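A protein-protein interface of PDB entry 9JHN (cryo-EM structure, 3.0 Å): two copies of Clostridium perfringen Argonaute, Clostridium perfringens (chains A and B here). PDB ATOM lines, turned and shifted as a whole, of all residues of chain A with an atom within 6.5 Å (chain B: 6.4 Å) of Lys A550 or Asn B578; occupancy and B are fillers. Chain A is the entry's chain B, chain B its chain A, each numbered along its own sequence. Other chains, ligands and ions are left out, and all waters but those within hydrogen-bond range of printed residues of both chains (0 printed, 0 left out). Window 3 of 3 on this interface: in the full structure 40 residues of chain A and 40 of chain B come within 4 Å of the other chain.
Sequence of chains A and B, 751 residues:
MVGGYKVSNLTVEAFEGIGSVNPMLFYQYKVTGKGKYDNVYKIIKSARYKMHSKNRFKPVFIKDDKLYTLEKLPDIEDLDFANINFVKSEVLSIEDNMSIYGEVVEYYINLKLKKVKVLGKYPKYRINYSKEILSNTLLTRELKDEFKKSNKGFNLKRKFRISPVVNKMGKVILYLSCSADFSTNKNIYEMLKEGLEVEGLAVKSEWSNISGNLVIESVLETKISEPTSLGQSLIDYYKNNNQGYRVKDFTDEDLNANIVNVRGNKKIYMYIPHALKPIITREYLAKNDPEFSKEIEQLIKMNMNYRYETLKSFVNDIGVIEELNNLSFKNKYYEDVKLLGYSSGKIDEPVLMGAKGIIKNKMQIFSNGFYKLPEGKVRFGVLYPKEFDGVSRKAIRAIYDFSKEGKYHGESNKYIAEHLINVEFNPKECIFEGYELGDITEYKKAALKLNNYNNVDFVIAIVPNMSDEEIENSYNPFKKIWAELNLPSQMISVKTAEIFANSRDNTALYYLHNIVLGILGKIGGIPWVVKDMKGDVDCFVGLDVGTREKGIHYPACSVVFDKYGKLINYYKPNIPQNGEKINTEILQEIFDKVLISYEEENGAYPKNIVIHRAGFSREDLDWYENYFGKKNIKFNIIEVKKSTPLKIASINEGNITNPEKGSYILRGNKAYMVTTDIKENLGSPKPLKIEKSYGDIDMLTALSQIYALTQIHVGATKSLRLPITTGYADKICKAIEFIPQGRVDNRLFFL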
ATOM      1  N   SER A 211      -0.758   7.129 -23.606  1.00  0.00           N
ATOM      2  CA  SER A 211      -0.060   5.868 -23.849  1.00  0.00           C
ATOM      3  C   SER A 211       0.811   5.570 -22.636  1.00  0.00           C
ATOM      4  O   SER A 211       1.919   6.093 -22.505  1.00  0.00           O
ATOM      5  CB  SER A 211       0.758   5.935 -25.134  1.00  0.00           C
ATOM      6  OG  SER A 211       1.821   6.861 -25.014  1.00  0.00           O
ATOM      7  N   THR A 547      16.428   0.181 -28.173  1.00  0.00           N
ATOM      8  CA  THR A 547      15.830   0.983 -27.108  1.00  0.00           C
ATOM      9  C   THR A 547      14.981   0.071 -26.219  1.00  0.00           C
ATOM     10  O   THR A 547      13.982  -0.502 -26.658  1.00  0.00           O
ATOM     11  CB  THR A 547      15.050   2.171 -27.692  1.00  0.00           C
ATOM     12  OG1 THR A 547      14.015   1.705 -28.568  1.00  0.00           O
ATOM     13  CG2 THR A 547      15.948   3.214 -28.377  1.00  0.00           C
ATOM     14  N   ARG A 548      15.399  -0.104 -24.967  1.00  0.00           N
ATOM     15  CA  ARG A 548      14.628  -0.960 -24.076  1.00  0.00           C
ATOM     16  C   ARG A 548      13.360  -0.258 -23.605  1.00  0.00           C
ATOM     17  O   ARG A 548      12.247  -0.745 -23.838  1.00  0.00           O
ATOM     18  CB  ARG A 548      15.473  -1.404 -22.881  1.00  0.00           C
ATOM     19  CG  ARG A 548      14.759  -2.456 -22.042  1.00  0.00           C
ATOM     20  CD  ARG A 548      15.533  -2.907 -20.817  1.00  0.00           C
ATOM     21  NE  ARG A 548      15.622  -1.865 -19.798  1.00  0.00           N
ATOM     22  CZ  ARG A 548      16.272  -2.002 -18.646  1.00  0.00           C
ATOM     23  NH1 ARG A 548      16.868  -3.149 -18.359  1.00  0.00           N
ATOM     24  NH2 ARG A 548      16.310  -1.003 -17.775  1.00  0.00           N
ATOM     25  N   GLU A 549      13.502   0.897 -22.960  1.00  0.00           N
ATOM     26  CA  GLU A 549      12.363   1.624 -22.421  1.00  0.00           C
ATOM     27  C   GLU A 549      12.352   3.034 -22.998  1.00  0.00           C
ATOM     28  O   GLU A 549      13.110   3.364 -23.915  1.00  0.00           O
ATOM     29  CB  GLU A 549      12.403   1.660 -20.890  1.00  0.00           C
ATOM     30  CG  GLU A 549      12.125   0.339 -20.212  1.00  0.00           C
ATOM     31  CD  GLU A 549      12.110   0.468 -18.700  1.00  0.00           C
ATOM     32  OE1 GLU A 549      12.471   1.551 -18.190  1.00  0.00           O
ATOM     33  OE2 GLU A 549      11.726  -0.507 -18.020  1.00  0.00           O
ATOM     34  N   LYS A 550      11.474   3.868 -22.453  1.00  0.00           N
ATOM     35  CA  LYS A 550      11.415   5.274 -22.823  1.00  0.00           C
ATOM     36  C   LYS A 550      12.549   6.028 -22.143  1.00  0.00           C
ATOM     37  O   LYS A 550      12.561   6.165 -20.915  1.00  0.00           O
ATOM     38  CB  LYS A 550      10.067   5.866 -22.426  1.00  0.00           C
ATOM     39  CG  LYS A 550       9.883   7.310 -22.839  1.00  0.00           C
ATOM     40  CD  LYS A 550       8.499   7.801 -22.479  1.00  0.00           C
ATOM     41  CE  LYS A 550       8.285   9.230 -22.929  1.00  0.00           C
ATOM     42  NZ  LYS A 550       6.912   9.695 -22.592  1.00  0.00           N
ATOM     43  N   GLY A 551      13.493   6.524 -22.936  1.00  0.00           N
ATOM     44  CA  GLY A 551      14.627   7.250 -22.405  1.00  0.00           C
ATOM     45  C   GLY A 551      15.887   6.433 -22.249  1.00  0.00           C
ATOM     46  O   GLY A 551      16.923   6.989 -21.868  1.00  0.00           O
ATOM     47  N   ILE A 552      15.834   5.137 -22.536  1.00  0.00           N
ATOM     48  CA  ILE A 552      16.984   4.250 -22.448  1.00  0.00           C
ATOM     49  C   ILE A 552      17.270   3.712 -23.838  1.00  0.00           C
ATOM     50  O   ILE A 552      16.410   3.065 -24.445  1.00  0.00           O
ATOM     51  CB  ILE A 552      16.729   3.093 -21.468  1.00  0.00           C
ATOM     52  CG1 ILE A 552      16.571   3.619 -20.041  1.00  0.00           C
ATOM     53  CG2 ILE A 552      17.831   2.049 -21.572  1.00  0.00           C
ATOM     54  CD1 ILE A 552      16.080   2.574 -19.068  1.00  0.00           C
ATOM     55  N   HIS B 553      22.255   9.752 -19.972  1.00  0.00           N
ATOM     56  CA  HIS B 553      22.574   9.717 -18.556  1.00  0.00           C
ATOM     57  C   HIS B 553      23.735   8.767 -18.330  1.00  0.00           C
ATOM     58  O   HIS B 553      23.775   7.678 -18.911  1.00  0.00           O
ATOM     59  CB  HIS B 553      21.372   9.307 -17.711  1.00  0.00           C
ATOM     60  CG  HIS B 553      20.299  10.343 -17.668  1.00  0.00           C
ATOM     61  ND1 HIS B 553      19.241  10.357 -18.549  1.00  0.00           N
ATOM     62  CD2 HIS B 553      20.145  11.430 -16.877  1.00  0.00           C
ATOM     63  CE1 HIS B 553      18.467  11.394 -18.285  1.00  0.00           C
ATOM     64  NE2 HIS B 553      18.996  12.064 -17.278  1.00  0.00           N
ATOM     65  N   PRO B 576      22.114   2.093 -19.404  1.00  0.00           N
ATOM     66  CA  PRO B 576      21.723   3.416 -18.920  1.00  0.00           C
ATOM     67  C   PRO B 576      20.333   3.360 -18.318  1.00  0.00           C
ATOM     68  O   PRO B 576      19.623   2.360 -18.423  1.00  0.00           O
ATOM     69  CB  PRO B 576      21.747   4.274 -20.185  1.00  0.00           C
ATOM     70  CG  PRO B 576      21.460   3.317 -21.265  1.00  0.00           C
ATOM     71  CD  PRO B 576      22.101   2.023 -20.871  1.00  0.00           C
ATOM     72  N   GLN B 577      19.935   4.452 -17.686  1.00  0.00           N
ATOM     73  CA  GLN B 577      18.636   4.461 -17.045  1.00  0.00           C
ATOM     74  C   GLN B 577      17.876   5.743 -17.359  1.00  0.00           C
ATOM     75  O   GLN B 577      18.300   6.563 -18.176  1.00  0.00           O
ATOM     76  CB  GLN B 577      18.788   4.257 -15.545  1.00  0.00           C
ATOM     77  CG  GLN B 577      19.470   5.374 -14.831  1.00  0.00           C
ATOM     78  CD  GLN B 577      19.610   5.066 -13.373  1.00  0.00           C
ATOM     79  OE1 GLN B 577      19.293   3.968 -12.927  1.00  0.00           O
ATOM     80  NE2 GLN B 577      20.027   6.046 -12.608  1.00  0.00           N
ATOM     81  N   ASN B 578      16.723   5.902 -16.715  1.00  0.00           N
ATOM     82  CA  ASN B 578      15.853   7.047 -16.942  1.00  0.00           C
ATOM     83  C   ASN B 578      16.126   8.096 -15.871  1.00  0.00           C
ATOM     84  O   ASN B 578      15.359   8.237 -14.915  1.00  0.00           O
ATOM     85  CB  ASN B 578      14.390   6.620 -16.935  1.00  0.00           C
ATOM     86  CG  ASN B 578      14.070   5.629 -18.033  1.00  0.00           C
ATOM     87  OD1 ASN B 578      13.668   4.496 -17.770  1.00  0.00           O
ATOM     88  ND2 ASN B 578      14.264   6.046 -19.275  1.00  0.00           N
ATOM     89  N   GLY B 579      17.223   8.820 -16.029  1.00  0.00           N
ATOM     90  CA  GLY B 579      17.447   9.967 -15.190  1.00  0.00           C
ATOM     91  C   GLY B 579      17.953   9.640 -13.802  1.00  0.00           C
ATOM     92  O   GLY B 579      18.535   8.591 -13.536  1.00  0.00           O
ATOM     93  N   GLU B 580      17.682  10.568 -12.894  1.00  0.00           N
ATOM     94  CA  GLU B 580      18.251  10.567 -11.555  1.00  0.00           C
ATOM     95  C   GLU B 580      17.603   9.546 -10.632  1.00  0.00           C
ATOM     96  O   GLU B 580      18.017   9.424  -9.477  1.00  0.00           O
ATOM     97  CB  GLU B 580      18.123  11.969 -10.966  1.00  0.00           C
ATOM     98  CG  GLU B 580      18.728  13.020 -11.880  1.00  0.00           C
ATOM     99  CD  GLU B 580      20.229  12.875 -12.033  1.00  0.00           C
ATOM    100  OE1 GLU B 580      20.901  12.546 -11.029  1.00  0.00           O
ATOM    101  OE2 GLU B 580      20.732  13.068 -13.161  1.00  0.00           O
ATOM    102  N   LYS B 581      16.601   8.822 -11.112  1.00  0.00           N
ATOM    103  CA  LYS B 581      15.993   7.722 -10.382  1.00  0.00           C
ATOM    104  C   LYS B 581      16.750   6.451 -10.734  1.00  0.00           C
ATOM    105  O   LYS B 581      16.829   6.077 -11.907  1.00  0.00           O
ATOM    106  CB  LYS B 581      14.521   7.602 -10.761  1.00  0.00           C
ATOM    107  CG  LYS B 581      13.747   6.497 -10.078  1.00  0.00           C
ATOM    108  CD  LYS B 581      13.394   6.849  -8.652  1.00  0.00           C
ATOM    109  CE  LYS B 581      12.437   5.815  -8.086  1.00  0.00           C
ATOM    110  NZ  LYS B 581      12.014   6.098  -6.693  1.00  0.00           N
ATOM    111  N   ILE B 582      17.323   5.800  -9.731  1.00  0.00           N
ATOM    112  CA  ILE B 582      17.946   4.498  -9.938  1.00  0.00           C
ATOM    113  C   ILE B 582      16.871   3.430  -9.788  1.00  0.00           C
ATOM    114  O   ILE B 582      16.163   3.389  -8.778  1.00  0.00           O
ATOM    115  CB  ILE B 582      19.102   4.273  -8.957  1.00  0.00           C
ATOM    116  CG1 ILE B 582      20.229   5.267  -9.203  1.00  0.00           C
ATOM    117  CG2 ILE B 582      19.651   2.920  -9.125  1.00  0.00           C
ATOM    118  CD1 ILE B 582      21.302   5.237  -8.145  1.00  0.00           C
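The side-chain amide oxygen (OD1) of Asn B578 sits close to the side-chain carboxylate (OE1) of Glu A549 (3.2 Å).
The backbone carbonyl oxygen (O) of Lys A550 lies close to the side-chain amide nitrogen (ND2) of Asn B578, 2.4 Å away.
The side-chain amide nitrogen (NE2) of Gln B577 sits at hydrogen-bond distance from the backbone carbonyl oxygen (O) of Gly B579, at 3.1 Å.
NE2 of Gln B577 lies within hydrogen-bond range of O of Lys B581.
Of the 7 printed residues of chain A, 4 touch a printed residue of chain B.
Hydrophobic or aromatic side chains of chain A within 4 Å of the printed part of chain B: Ile A552.
Among the printed residues, 7 pairs touch across the chains.
Among the printed residues, merely in contact across the chains: Gly A551 with Gln B577, Gly A551 with Asn B578, Ile A552 with Pro B576, Ile A552 with Gln B577 and Ile A552 with Asn B578.
No position is printed for both chains.
Of the 7 pairs that touch across the chains among the printed residues, none has its exchanged pair printed and touching as well.
Of the printed residues of chain B, Glu A549 touches Asn B578.
Of chain B, only Asn B578 (2.4 Å) comes within 4 Å of Lys A550.
Of the printed residues of chain B, Gly A551 touches Gln B577 and Asn B578.
Of the printed residues of chain A, Gln B577 touches Gly A551 and Ile A552.
Of the printed residues of chain A, Asn B578 touches Glu A549 (3.2 Å), Lys A550 (2.4 Å), Gly A551 (3.4 Å) and Ile A552 (3.3 Å).
Gly B579 touches none of the printed residues of chain A.
The nearest printed residue of chain B that does not touch Lys A550 is Gln B577 (6.4 Å).
The nearest printed residue of chain B that does not touch Glu A549 is Gln B577 (6.9 Å).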
